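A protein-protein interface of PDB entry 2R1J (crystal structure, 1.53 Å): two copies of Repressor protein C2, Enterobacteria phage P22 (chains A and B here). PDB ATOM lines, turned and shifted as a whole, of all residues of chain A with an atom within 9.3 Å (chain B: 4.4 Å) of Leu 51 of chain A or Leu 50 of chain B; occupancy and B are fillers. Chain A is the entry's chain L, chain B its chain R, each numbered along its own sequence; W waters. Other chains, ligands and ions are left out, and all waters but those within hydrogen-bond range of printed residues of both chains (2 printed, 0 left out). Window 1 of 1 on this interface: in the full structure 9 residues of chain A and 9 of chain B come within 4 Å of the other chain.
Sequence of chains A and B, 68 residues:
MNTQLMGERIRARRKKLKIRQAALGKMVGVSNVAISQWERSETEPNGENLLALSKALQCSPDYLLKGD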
ATOM      1  N   MET A   6      35.854   5.648 -26.684  1.00  0.00           N
ATOM      2  CA  MET A   6      34.758   5.331 -27.596  1.00  0.00           C
ATOM      3  C   MET A   6      35.173   5.628 -29.036  1.00  0.00           C
ATOM      4  O   MET A   6      34.866   4.854 -29.938  1.00  0.00           O
ATOM      5  CB  MET A   6      33.493   6.152 -27.250  1.00  0.00           C
ATOM      6  CG  MET A   6      32.392   6.054 -28.318  1.00  0.00           C
ATOM      7  SD  MET A   6      30.771   6.725 -27.792  1.00  0.00           S
ATOM      8  CE  MET A   6      31.328   8.171 -27.032  1.00  0.00           C
ATOM      9  N   MET A  27      25.033   8.059 -43.544  1.00  0.00           N
ATOM     10  CA  MET A  27      24.206   7.038 -42.918  1.00  0.00           C
ATOM     11  C   MET A  27      23.597   7.505 -41.586  1.00  0.00           C
ATOM     12  O   MET A  27      22.451   7.186 -41.274  1.00  0.00           O
ATOM     13  CB  MET A  27      25.036   5.783 -42.657  1.00  0.00           C
ATOM     14  CG  MET A  27      25.474   5.000 -43.899  1.00  0.00           C
ATOM     15  SD  MET A  27      26.624   3.657 -43.388  1.00  0.00           S
ATOM     16  CE  MET A  27      25.422   2.440 -42.871  1.00  0.00           C
ATOM     17  N   VAL A  28      24.385   8.249 -40.808  1.00  0.00           N
ATOM     18  CA  VAL A  28      23.968   8.761 -39.487  1.00  0.00           C
ATOM     19  C   VAL A  28      23.190  10.071 -39.560  1.00  0.00           C
ATOM     20  O   VAL A  28      22.327  10.330 -38.715  1.00  0.00           O
ATOM     21  CB  VAL A  28      25.222   8.966 -38.591  1.00  0.00           C
ATOM     22  CG1 VAL A  28      24.853   9.588 -37.236  1.00  0.00           C
ATOM     23  CG2 VAL A  28      25.921   7.622 -38.412  1.00  0.00           C
ATOM     24  N   TRP A  38      34.218  12.604 -33.466  1.00  0.00           N
ATOM     25  CA  TRP A  38      33.909  11.504 -32.569  1.00  0.00           C
ATOM     26  C   TRP A  38      35.071  10.511 -32.525  1.00  0.00           C
ATOM     27  O   TRP A  38      35.439  10.024 -31.451  1.00  0.00           O
ATOM     28  CB  TRP A  38      32.667  10.734 -33.008  1.00  0.00           C
ATOM     29  CG  TRP A  38      31.434  11.583 -33.045  1.00  0.00           C
ATOM     30  CD1 TRP A  38      31.244  12.790 -32.413  1.00  0.00           C
ATOM     31  CD2 TRP A  38      30.241  11.302 -33.759  1.00  0.00           C
ATOM     32  NE1 TRP A  38      29.988  13.285 -32.715  1.00  0.00           N
ATOM     33  CE2 TRP A  38      29.349  12.391 -33.537  1.00  0.00           C
ATOM     34  CE3 TRP A  38      29.830  10.242 -34.568  1.00  0.00           C
ATOM     35  CZ2 TRP A  38      28.073  12.443 -34.108  1.00  0.00           C
ATOM     36  CZ3 TRP A  38      28.560  10.287 -35.144  1.00  0.00           C
ATOM     37  CH2 TRP A  38      27.690  11.383 -34.912  1.00  0.00           C
ATOM     38  N   PRO A  45      29.027  11.781 -29.548  1.00  0.00           N
ATOM     39  CA  PRO A  45      27.729  11.968 -30.189  1.00  0.00           C
ATOM     40  C   PRO A  45      26.606  12.242 -29.190  1.00  0.00           C
ATOM     41  O   PRO A  45      26.612  11.701 -28.079  1.00  0.00           O
ATOM     42  CB  PRO A  45      27.503  10.651 -30.931  1.00  0.00           C
ATOM     43  CG  PRO A  45      28.304   9.651 -30.129  1.00  0.00           C
ATOM     44  CD  PRO A  45      29.527  10.396 -29.690  1.00  0.00           C
ATOM     45  N   ASN A  46      25.649  13.057 -29.621  1.00  0.00           N
ATOM     46  CA  ASN A  46      24.520  13.358 -28.758  1.00  0.00           C
ATOM     47  C   ASN A  46      23.574  12.139 -28.752  1.00  0.00           C
ATOM     48  O   ASN A  46      23.871  11.112 -29.354  1.00  0.00           O
ATOM     49  CB  ASN A  46      23.821  14.667 -29.200  1.00  0.00           C
ATOM     50  CG  ASN A  46      23.100  14.560 -30.524  1.00  0.00           C
ATOM     51  OD1 ASN A  46      22.755  13.466 -30.973  1.00  0.00           O
ATOM     52  ND2 ASN A  46      22.841  15.700 -31.146  1.00  0.00           N
ATOM     53  N   GLY A  47      22.443  12.241 -28.067  1.00  0.00           N
ATOM     54  CA  GLY A  47      21.556  11.093 -27.947  1.00  0.00           C
ATOM     55  C   GLY A  47      21.061  10.485 -29.242  1.00  0.00           C
ATOM     56  O   GLY A  47      21.201   9.282 -29.491  1.00  0.00           O
ATOM     57  N   GLU A  48      20.455  11.320 -30.068  1.00  0.00           N
ATOM     58  CA  GLU A  48      19.916  10.834 -31.335  1.00  0.00           C
ATOM     59  C   GLU A  48      21.038  10.302 -32.219  1.00  0.00           C
ATOM     60  O   GLU A  48      20.907   9.249 -32.872  1.00  0.00           O
ATOM     61  CB  GLU A  48      19.192  11.986 -32.056  1.00  0.00           C
ATOM     62  CG  GLU A  48      18.792  11.701 -33.505  1.00  0.00           C
ATOM     63  CD  GLU A  48      17.819  12.743 -34.056  1.00  0.00           C
ATOM     64  OE1 GLU A  48      17.710  13.830 -33.440  1.00  0.00           O
ATOM     65  OE2 GLU A  48      17.171  12.477 -35.105  1.00  0.00           O
ATOM     66  N   ASN A  49      22.153  11.020 -32.230  1.00  0.00           N
ATOM     67  CA  ASN A  49      23.249  10.622 -33.086  1.00  0.00           C
ATOM     68  C   ASN A  49      23.933   9.335 -32.613  1.00  0.00           C
ATOM     69  O   ASN A  49      24.365   8.527 -33.452  1.00  0.00           O
ATOM     70  CB  ASN A  49      24.250  11.763 -33.236  1.00  0.00           C
ATOM     71  CG  ASN A  49      23.702  12.910 -34.079  1.00  0.00           C
ATOM     72  OD1 ASN A  49      22.765  12.729 -34.883  1.00  0.00           O
ATOM     73  ND2 ASN A  49      24.280  14.097 -33.921  1.00  0.00           N
ATOM     74  N   LEU A  50      24.050   9.126 -31.304  1.00  0.00           N
ATOM     75  CA  LEU A  50      24.670   7.896 -30.838  1.00  0.00           C
ATOM     76  C   LEU A  50      23.810   6.708 -31.266  1.00  0.00           C
ATOM     77  O   LEU A  50      24.340   5.681 -31.709  1.00  0.00           O
ATOM     78  CB  LEU A  50      24.847   7.889 -29.308  1.00  0.00           C
ATOM     79  CG  LEU A  50      25.369   6.584 -28.673  1.00  0.00           C
ATOM     80  CD1 LEU A  50      26.775   6.233 -29.152  1.00  0.00           C
ATOM     81  CD2 LEU A  50      25.345   6.782 -27.162  1.00  0.00           C
ATOM     82  N   LEU A  51      22.498   6.826 -31.140  1.00  0.00           N
ATOM     83  CA  LEU A  51      21.647   5.708 -31.539  1.00  0.00           C
ATOM     84  C   LEU A  51      21.768   5.448 -33.042  1.00  0.00           C
ATOM     85  O   LEU A  51      21.915   4.293 -33.467  1.00  0.00           O
ATOM     86  CB  LEU A  51      20.210   5.975 -31.121  1.00  0.00           C
ATOM     87  CG  LEU A  51      19.873   5.368 -29.752  1.00  0.00           C
ATOM     88  CD1 LEU A  51      19.813   3.834 -29.918  1.00  0.00           C
ATOM     89  CD2 LEU A  51      20.912   5.712 -28.704  1.00  0.00           C
ATOM     90  N   ALA A  52      21.750   6.500 -33.857  1.00  0.00           N
ATOM     91  CA  ALA A  52      21.873   6.303 -35.305  1.00  0.00           C
ATOM     92  C   ALA A  52      23.232   5.717 -35.682  1.00  0.00           C
ATOM     93  O   ALA A  52      23.342   4.920 -36.625  1.00  0.00           O
ATOM     94  CB  ALA A  52      21.629   7.639 -36.049  1.00  0.00           C
ATOM     95  N   LEU A  53      24.265   6.118 -34.947  1.00  0.00           N
ATOM     96  CA  LEU A  53      25.613   5.642 -35.176  1.00  0.00           C
ATOM     97  C   LEU A  53      25.704   4.138 -34.849  1.00  0.00           C
ATOM     98  O   LEU A  53      26.293   3.356 -35.611  1.00  0.00           O
ATOM     99  CB  LEU A  53      26.590   6.429 -34.297  1.00  0.00           C
ATOM    100  CG  LEU A  53      28.061   6.004 -34.324  1.00  0.00           C
ATOM    101  CD1 LEU A  53      28.649   6.253 -35.718  1.00  0.00           C
ATOM    102  CD2 LEU A  53      28.844   6.806 -33.266  1.00  0.00           C
ATOM    103  N   SER A  54      25.109   3.739 -33.735  1.00  0.00           N
ATOM    104  CA  SER A  54      25.140   2.335 -33.330  1.00  0.00           C
ATOM    105  C   SER A  54      24.469   1.474 -34.412  1.00  0.00           C
ATOM    106  O   SER A  54      24.936   0.374 -34.706  1.00  0.00           O
ATOM    107  CB  SER A  54      24.437   2.152 -31.983  1.00  0.00           C
ATOM    108  OG  SER A  54      23.053   2.418 -32.077  1.00  0.00           O
ATOM    109  N   LYS A  55      23.387   1.964 -35.002  1.00  0.00           N
ATOM    110  CA  LYS A  55      22.713   1.195 -36.053  1.00  0.00           C
ATOM    111  C   LYS A  55      23.596   1.114 -37.304  1.00  0.00           C
ATOM    112  O   LYS A  55      23.780   0.029 -37.874  1.00  0.00           O
ATOM    113  CB  LYS A  55      21.361   1.817 -36.387  1.00  0.00           C
ATOM    114  CG  LYS A  55      20.372   1.642 -35.269  1.00  0.00           C
ATOM    115  CD  LYS A  55      19.081   2.358 -35.532  1.00  0.00           C
ATOM    116  CE  LYS A  55      18.138   2.131 -34.363  1.00  0.00           C
ATOM    117  NZ  LYS A  55      18.796   2.475 -33.053  1.00  0.00           N
ATOM    118  N   ALA A  56      24.159   2.239 -37.724  1.00  0.00           N
ATOM    119  CA  ALA A  56      25.032   2.251 -38.904  1.00  0.00           C
ATOM    120  C   ALA A  56      26.241   1.335 -38.742  1.00  0.00           C
ATOM    121  O   ALA A  56      26.683   0.710 -39.713  1.00  0.00           O
ATOM    122  CB  ALA A  56      25.503   3.686 -39.202  1.00  0.00           C
ATOM    123  N   LEU A  57      26.772   1.239 -37.526  1.00  0.00           N
ATOM    124  CA  LEU A  57      27.941   0.398 -37.269  1.00  0.00           C
ATOM    125  C   LEU A  57      27.574  -1.015 -36.829  1.00  0.00           C
ATOM    126  O   LEU A  57      28.445  -1.799 -36.503  1.00  0.00           O
ATOM    127  CB  LEU A  57      28.847   1.035 -36.216  1.00  0.00           C
ATOM    128  CG  LEU A  57      29.446   2.400 -36.574  1.00  0.00           C
ATOM    129  CD1 LEU A  57      30.315   2.907 -35.410  1.00  0.00           C
ATOM    130  CD2 LEU A  57      30.279   2.281 -37.847  1.00  0.00           C
ATOM    131  N   GLN A  58      26.283  -1.308 -36.784  1.00  0.00           N
ATOM    132  CA  GLN A  58      25.789  -2.638 -36.421  1.00  0.00           C
ATOM    133  C   GLN A  58      26.197  -3.120 -35.031  1.00  0.00           C
ATOM    134  O   GLN A  58      26.599  -4.268 -34.850  1.00  0.00           O
ATOM    135  CB  GLN A  58      26.245  -3.648 -37.485  1.00  0.00           C
ATOM    136  CG  GLN A  58      25.964  -3.160 -38.890  1.00  0.00           C
ATOM    137  CD  GLN A  58      26.440  -4.109 -39.975  1.00  0.00           C
ATOM    138  OE1 GLN A  58      26.345  -3.795 -41.159  1.00  0.00           O
ATOM    139  NE2 GLN A  58      26.946  -5.271 -39.580  1.00  0.00           N
ATOM    140  N   CYS A  59      26.082  -2.252 -34.035  1.00  0.00           N
ATOM    141  CA  CYS A  59      26.440  -2.644 -32.687  1.00  0.00           C
ATOM    142  C   CYS A  59      25.558  -1.901 -31.694  1.00  0.00           C
ATOM    143  O   CYS A  59      24.709  -1.106 -32.086  1.00  0.00           O
ATOM    144  CB  CYS A  59      27.910  -2.337 -32.426  1.00  0.00           C
ATOM    145  SG  CYS A  59      28.336  -0.569 -32.525  1.00  0.00           S
ATOM    146  N   SER A  60      25.748  -2.148 -30.407  1.00  0.00           N
ATOM    147  CA  SER A  60      24.921  -1.459 -29.426  1.00  0.00           C
ATOM    148  C   SER A  60      25.576  -0.147 -28.991  1.00  0.00           C
ATOM    149  O   SER A  60      26.790   0.024 -29.098  1.00  0.00           O
ATOM    150  CB  SER A  60      24.703  -2.340 -28.191  1.00  0.00           C
ATOM    151  OG  SER A  60      25.884  -2.395 -27.410  1.00  0.00           O
ATOM    152  N   PRO A  61      24.764   0.803 -28.511  1.00  0.00           N
ATOM    153  CA  PRO A  61      25.298   2.094 -28.050  1.00  0.00           C
ATOM    154  C   PRO A  61      26.231   1.831 -26.855  1.00  0.00           C
ATOM    155  O   PRO A  61      27.226   2.516 -26.656  1.00  0.00           O
ATOM    156  CB  PRO A  61      24.048   2.855 -27.598  1.00  0.00           C
ATOM    157  CG  PRO A  61      22.938   2.248 -28.376  1.00  0.00           C
ATOM    158  CD  PRO A  61      23.294   0.772 -28.426  1.00  0.00           C
ATOM    159  N   ASP A  62      25.861   0.846 -26.041  1.00  0.00           N
ATOM    160  CA  ASP A  62      26.644   0.471 -24.871  1.00  0.00           C
ATOM    161  C   ASP A  62      28.048   0.029 -25.262  1.00  0.00           C
ATOM    162  O   ASP A  62      29.017   0.361 -24.586  1.00  0.00           O
ATOM    163  CB  ASP A  62      25.938  -0.654 -24.147  1.00  0.00           C
ATOM    164  CG  ASP A  62      24.509  -0.303 -23.825  1.00  0.00           C
ATOM    165  OD1 ASP A  62      24.303   0.303 -22.751  1.00  0.00           O
ATOM    166  OD2 ASP A  62      23.609  -0.600 -24.665  1.00  0.00           O
ATOM    167  N   LEU A  64      29.777   0.981 -27.906  1.00  0.00           N
ATOM    168  CA  LEU A  64      30.544   2.163 -28.274  1.00  0.00           C
ATOM    169  C   LEU A  64      30.947   2.968 -27.043  1.00  0.00           C
ATOM    170  O   LEU A  64      32.098   3.354 -26.897  1.00  0.00           O
ATOM    171  CB  LEU A  64      29.740   3.068 -29.229  1.00  0.00           C
ATOM    172  CG  LEU A  64      29.474   2.463 -30.614  1.00  0.00           C
ATOM    173  CD1 LEU A  64      28.638   3.421 -31.463  1.00  0.00           C
ATOM    174  CD2 LEU A  64      30.803   2.172 -31.286  1.00  0.00           C
ATOM    175  N   LEU A  65      29.995   3.201 -26.152  1.00  0.00           N
ATOM    176  CA  LEU A  65      30.261   3.999 -24.951  1.00  0.00           C
ATOM    177  C   LEU A  65      31.264   3.425 -23.954  1.00  0.00           C
ATOM    178  O   LEU A  65      32.164   4.132 -23.500  1.00  0.00           O
ATOM    179  CB  LEU A  65      28.957   4.268 -24.207  1.00  0.00           C
ATOM    180  CG  LEU A  65      28.015   5.352 -24.748  1.00  0.00           C
ATOM    181  CD1 LEU A  65      26.681   5.310 -23.972  1.00  0.00           C
ATOM    182  CD2 LEU A  65      28.687   6.728 -24.596  1.00  0.00           C
ATOM    183  N   PRO B  45      18.823  14.694 -23.946  1.00  0.00           N
ATOM    184  CA  PRO B  45      20.034  14.136 -23.314  1.00  0.00           C
ATOM    185  C   PRO B  45      21.122  13.789 -24.307  1.00  0.00           C
ATOM    186  O   PRO B  45      20.824  13.400 -25.442  1.00  0.00           O
ATOM    187  CB  PRO B  45      19.513  12.905 -22.557  1.00  0.00           C
ATOM    188  CG  PRO B  45      18.228  12.564 -23.247  1.00  0.00           C
ATOM    189  CD  PRO B  45      17.633  13.864 -23.708  1.00  0.00           C
ATOM    190  N   ASN B  46      22.376  13.966 -23.885  1.00  0.00           N
ATOM    191  CA  ASN B  46      23.507  13.633 -24.742  1.00  0.00           C
ATOM    192  C   ASN B  46      23.638  12.071 -24.804  1.00  0.00           C
ATOM    193  O   ASN B  46      22.830  11.346 -24.231  1.00  0.00           O
ATOM    194  CB  ASN B  46      24.763  14.371 -24.230  1.00  0.00           C
ATOM    195  CG  ASN B  46      25.389  13.770 -22.983  1.00  0.00           C
ATOM    196  OD1 ASN B  46      25.077  12.640 -22.545  1.00  0.00           O
ATOM    197  ND2 ASN B  46      26.282  14.544 -22.376  1.00  0.00           N
ATOM    198  N   GLY B  47      24.643  11.561 -25.505  1.00  0.00           N
ATOM    199  CA  GLY B  47      24.734  10.110 -25.651  1.00  0.00           C
ATOM    200  C   GLY B  47      24.795   9.309 -24.365  1.00  0.00           C
ATOM    201  O   GLY B  47      23.955   8.442 -24.092  1.00  0.00           O
ATOM    202  N   GLU B  48      25.781   9.628 -23.540  1.00  0.00           N
ATOM    203  CA  GLU B  48      25.956   8.919 -22.283  1.00  0.00           C
ATOM    204  C   GLU B  48      24.745   9.076 -21.359  1.00  0.00           C
ATOM    205  O   GLU B  48      24.314   8.118 -20.699  1.00  0.00           O
ATOM    206  CB  GLU B  48      27.223   9.423 -21.590  1.00  0.00           C
ATOM    207  CG  GLU B  48      27.482   8.804 -20.240  1.00  0.00           C
ATOM    208  CD  GLU B  48      28.721   9.374 -19.578  1.00  0.00           C
ATOM    209  OE1 GLU B  48      29.081   8.900 -18.467  1.00  0.00           O
ATOM    210  OE2 GLU B  48      29.336  10.300 -20.164  1.00  0.00           O
ATOM    211  N   ASN B  49      24.185  10.284 -21.311  1.00  0.00           N
ATOM    212  CA  ASN B  49      23.038  10.495 -20.446  1.00  0.00           C
ATOM    213  C   ASN B  49      21.768   9.810 -20.944  1.00  0.00           C
ATOM    214  O   ASN B  49      20.924   9.411 -20.138  1.00  0.00           O
ATOM    215  CB  ASN B  49      22.776  12.018 -20.236  1.00  0.00           C
ATOM    216  CG  ASN B  49      23.898  12.699 -19.488  1.00  0.00           C
ATOM    217  OD1 ASN B  49      24.613  12.056 -18.697  1.00  0.00           O
ATOM    218  ND2 ASN B  49      24.059  14.007 -19.699  1.00  0.00           N
ATOM    219  N   LEU B  50      21.605   9.688 -22.262  1.00  0.00           N
ATOM    220  CA  LEU B  50      20.424   9.034 -22.816  1.00  0.00           C
ATOM    221  C   LEU B  50      20.480   7.564 -22.380  1.00  0.00           C
ATOM    222  O   LEU B  50      19.470   7.013 -21.954  1.00  0.00           O
ATOM    223  CB  LEU B  50      20.412   9.087 -24.362  1.00  0.00           C
ATOM    224  CG  LEU B  50      19.216   8.326 -25.004  1.00  0.00           C
ATOM    225  CD1 LEU B  50      17.887   8.781 -24.389  1.00  0.00           C
ATOM    226  CD2 LEU B  50      19.178   8.548 -26.494  1.00  0.00           C
ATOM    227  N   LEU B  51      21.655   6.944 -22.489  1.00  0.00           N
ATOM    228  CA  LEU B  51      21.756   5.534 -22.086  1.00  0.00           C
ATOM    229  C   LEU B  51      21.512   5.375 -20.583  1.00  0.00           C
ATOM    230  O   LEU B  51      20.763   4.485 -20.188  1.00  0.00           O
ATOM    231  CB  LEU B  51      23.104   4.959 -22.520  1.00  0.00           C
ATOM    232  CG  LEU B  51      23.052   4.280 -23.912  1.00  0.00           C
ATOM    233  CD1 LEU B  51      22.178   3.028 -23.811  1.00  0.00           C
ATOM    234  CD2 LEU B  51      22.451   5.186 -24.986  1.00  0.00           C
ATOM    235  N   ALA B  52      22.100   6.241 -19.748  1.00  0.00           N
ATOM    236  CA  ALA B  52      21.881   6.145 -18.311  1.00  0.00           C
ATOM    237  C   ALA B  52      20.426   6.371 -17.956  1.00  0.00           C
ATOM    238  O   ALA B  52      19.867   5.711 -17.058  1.00  0.00           O
ATOM    239  CB  ALA B  52      22.737   7.144 -17.574  1.00  0.00           C
ATOM    240  N   LEU B  53      19.799   7.326 -18.648  1.00  0.00           N
ATOM    241  CA  LEU B  53      18.402   7.628 -18.398  1.00  0.00           C
ATOM    242  C   LEU B  53      17.530   6.435 -18.791  1.00  0.00           C
ATOM    243  O   LEU B  53      16.596   6.104 -18.084  1.00  0.00           O
ATOM    244  CB  LEU B  53      17.973   8.872 -19.201  1.00  0.00           C
ATOM    245  CG  LEU B  53      16.488   9.217 -19.168  1.00  0.00           C
ATOM    246  CD1 LEU B  53      16.011   9.660 -17.760  1.00  0.00           C
ATOM    247  CD2 LEU B  53      16.256  10.355 -20.145  1.00  0.00           C
ATOM    248  N   SER B  54      17.846   5.792 -19.910  1.00  0.00           N
ATOM    249  CA  SER B  54      17.036   4.665 -20.350  1.00  0.00           C
ATOM    250  C   SER B  54      17.097   3.539 -19.322  1.00  0.00           C
ATOM    251  O   SER B  54      16.083   2.897 -19.056  1.00  0.00           O
ATOM    252  CB  SER B  54      17.459   4.173 -21.748  1.00  0.00           C
ATOM    253  OG  SER B  54      18.738   3.564 -21.748  1.00  0.00           O
ATOM    254  N   PRO B  61      16.519   3.162 -25.255  1.00  0.00           N
ATOM    255  CA  PRO B  61      16.799   4.537 -25.671  1.00  0.00           C
ATOM    256  C   PRO B  61      15.912   4.858 -26.871  1.00  0.00           C
ATOM    257  O   PRO B  61      15.479   5.984 -27.040  1.00  0.00           O
ATOM    258  CB  PRO B  61      18.265   4.490 -26.091  1.00  0.00           C
ATOM    259  CG  PRO B  61      18.836   3.359 -25.279  1.00  0.00           C
ATOM    260  CD  PRO B  61      17.740   2.336 -25.278  1.00  0.00           C
ATOM    261  N   ASP B  62      15.654   3.859 -27.723  1.00  0.00           N
ATOM    262  CA  ASP B  62      14.815   4.091 -28.902  1.00  0.00           C
ATOM    263  C   ASP B  62      13.399   4.473 -28.514  1.00  0.00           C
ATOM    264  O   ASP B  62      12.776   5.328 -29.162  1.00  0.00           O
ATOM    265  CB  ASP B  62      14.793   2.855 -29.811  1.00  0.00           C
ATOM    266  CG  ASP B  62      16.002   2.785 -30.732  1.00  0.00           C
ATOM    267  OD1 ASP B  62      16.576   1.685 -30.879  1.00  0.00           O
ATOM    268  OD2 ASP B  62      16.372   3.825 -31.325  1.00  0.00           O
ATOM    269  N   LEU B  64      12.474   6.094 -25.819  1.00  0.00           N
ATOM    270  CA  LEU B  64      12.454   7.506 -25.450  1.00  0.00           C
ATOM    271  C   LEU B  64      12.589   8.411 -26.662  1.00  0.00           C
ATOM    272  O   LEU B  64      11.846   9.362 -26.782  1.00  0.00           O
ATOM    273  CB  LEU B  64      13.561   7.839 -24.439  1.00  0.00           C
ATOM    274  CG  LEU B  64      13.450   7.050 -23.121  1.00  0.00           C
ATOM    275  CD1 LEU B  64      14.631   7.328 -22.218  1.00  0.00           C
ATOM    276  CD2 LEU B  64      12.170   7.444 -22.414  1.00  0.00           C
ATOM    277  N   LEU B  65      13.532   8.111 -27.551  1.00  0.00           N
ATOM    278  CA  LEU B  65      13.762   8.957 -28.719  1.00  0.00           C
ATOM    279  C   LEU B  65      12.593   9.052 -29.673  1.00  0.00           C
ATOM    280  O   LEU B  65      12.216  10.136 -30.060  1.00  0.00           O
ATOM    281  CB  LEU B  65      14.977   8.485 -29.511  1.00  0.00           C
ATOM    282  CG  LEU B  65      16.368   8.858 -28.998  1.00  0.00           C
ATOM    283  CD1 LEU B  65      17.419   8.102 -29.804  1.00  0.00           C
ATOM    284  CD2 LEU B  65      16.591  10.384 -29.132  1.00  0.00           C
HETATM  285  O   HOH W   1      21.087  15.370 -27.528  1.00  0.00           O
HETATM  286  O   HOH W   2      27.389  13.477 -26.046  1.00  0.00           O
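Asn 46 of chain A touches Gly 47 of chain B, and with the chains exchanged Gly 47 of chain A touches Asn 46 of chain B. Gly 47 of chain A touches its own counterpart, Gly 47 of chain B. Leu 51 of chain A touches Pro 61 of chain B, and with the chains exchanged Pro 61 of chain A touches Leu 51 of chain B. Leu 51 of chain A touches Asp 62 of chain B, and with the chains exchanged Asp 62 of chain A touches Leu 51 of chain B. Positions printed for both chains: 45, 46, 47, 48, 49, 50, 51, 52, 53, 54, 61, 62, 64 and 65.
Water W2 bridges the backbone carbonyl oxygen (O) of Pro 45 of chain A and the backbone NH (N) of Gly 47 of chain B. Water W1 bridges the backbone carbonyl oxygen of Pro 45 of chain B (2.9 Å) and the backbone NH of Gly 47 of chain A (3.5 Å).
Of the printed residues of chain B, Leu 51 of chain A touches Leu 50 (3.99 Å), Pro 61 (3.9 Å), Asp 62 (3.7 Å) and Leu 65 (3.7 Å). Printed residues of chain A within 4 Å of Leu 50 of chain B: Gly 47 (3.7 Å) and Leu 51 (3.99 Å). Of chain A, only Pro 45, Asn 46, Gly 47 and Leu 50 come within 4 Å of Gly 47 of chain B. Of the printed residues of chain A, Asp 62 of chain B touches Leu 51 (3.7 Å) and Lys 55 (3.2 Å). Of the printed residues of chain B, Pro 61 of chain A touches Leu 51 (3.8 Å). Of the printed residues of chain A, Pro 45 of chain B touches Gly 47 (3.3 Å). Printed residues of chain B within 4 Å of Leu 50 of chain A: Gly 47 and Leu 51. Ser 54 of chain A touches none of the printed residues of chain B. The nearest printed residue of chain A that does not touch Leu 50 of chain B is Glu 48 of chain A (4.7 Å). The nearest printed residue of chain B that does not touch Leu 50 of chain A is Glu 48 of chain B (4.6 Å).
The backbone carbonyl oxygen of Leu 51 of chain A is in hydrogen-bond range of the side-chain hydroxyl of Ser 54 of chain A (2.6 Å). O of Leu 51 of chain B is in hydrogen-bond range of OG of Ser 54 of chain B. The side-chain amide oxygen (OD1) of Asn 46 of chain A lies within hydrogen-bond range of the backbone NH (N) of Glu 48 of chain A, 3.3 Å away. The side-chain amide oxygen (OD1) of Asn 46 of chain A sits at hydrogen-bond distance from the backbone NH (N) of Asn 49 of chain A. The backbone NH (N) of Glu 48 of chain B is in hydrogen-bond range of the side-chain amide oxygen (OD1) of Asn 46 of chain B (3.2 Å). The side-chain amide oxygen of Asn 46 of chain B is in hydrogen-bond range of the backbone NH of Asn 49 of chain B (2.8 Å).
Printed residues of chain A that touch a printed residue of chain B: Pro 45, Asn 46, Gly 47, Leu 50, Leu 51, Lys 55, Pro 61, Asp 62 and Leu 65. Hydrophobic or aromatic side chains of chain A that line the printed part of chain B: Leu 50, Leu 51, Pro 61 and Leu 65. Among the printed residues, 18 pairs touch across the chains. Among the printed residues, Asp or Glu carboxylates within 4 Å of a Lys or Arg side-chain nitrogen of the other chain: Lys 55 of chain A with Asp 62 of chain B (3.2 Å).
Asn 46 of chain A touches Asn 46 of chain B. Gly 47 of chain A touches Leu 50 of chain B (O to CD2, 3.7 Å). Gly 47 of chain A touches Leu 65 of chain B (O to CD1, 3.97 Å). Leu 50 of chain A touches Leu 51 of chain B (CD2 to CD2, 3.96 Å). Leu 51 of chain A touches Leu 50 of chain B. Pro 61 of chain B touches Leu 51 of chain A (CB to CD2, 3.9 Å). Asp 62 of chain B touches Leu 51 of chain A (OD2 to CD1, 3.7 Å). Pro 61 of chain A touches Leu 51 of chain B. Asp 62 of chain A touches Leu 51 of chain B (OD1 to CD1, 3.6 Å). CD1 of Leu 65 of chain A touches CG of Leu 51 of chain B (3.8 Å).
The backbone NH of Gly 47 of chain B sits at hydrogen-bond distance from the backbone carbonyl oxygen of Pro 45 of chain A, 3.2 Å away. The side-chain amino group (NZ) of Lys 55 of chain A is in salt-bridge range of the side-chain carboxylate (OD1) of Asp 62 of chain B, 3.2 Å away. The backbone NH of Gly 47 of chain B lies close to the backbone NH of Gly 47 of chain A. The backbone NH of Gly 47 of chain A lies within hydrogen-bond range of the backbone carbonyl oxygen of Pro 45 of chain B.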
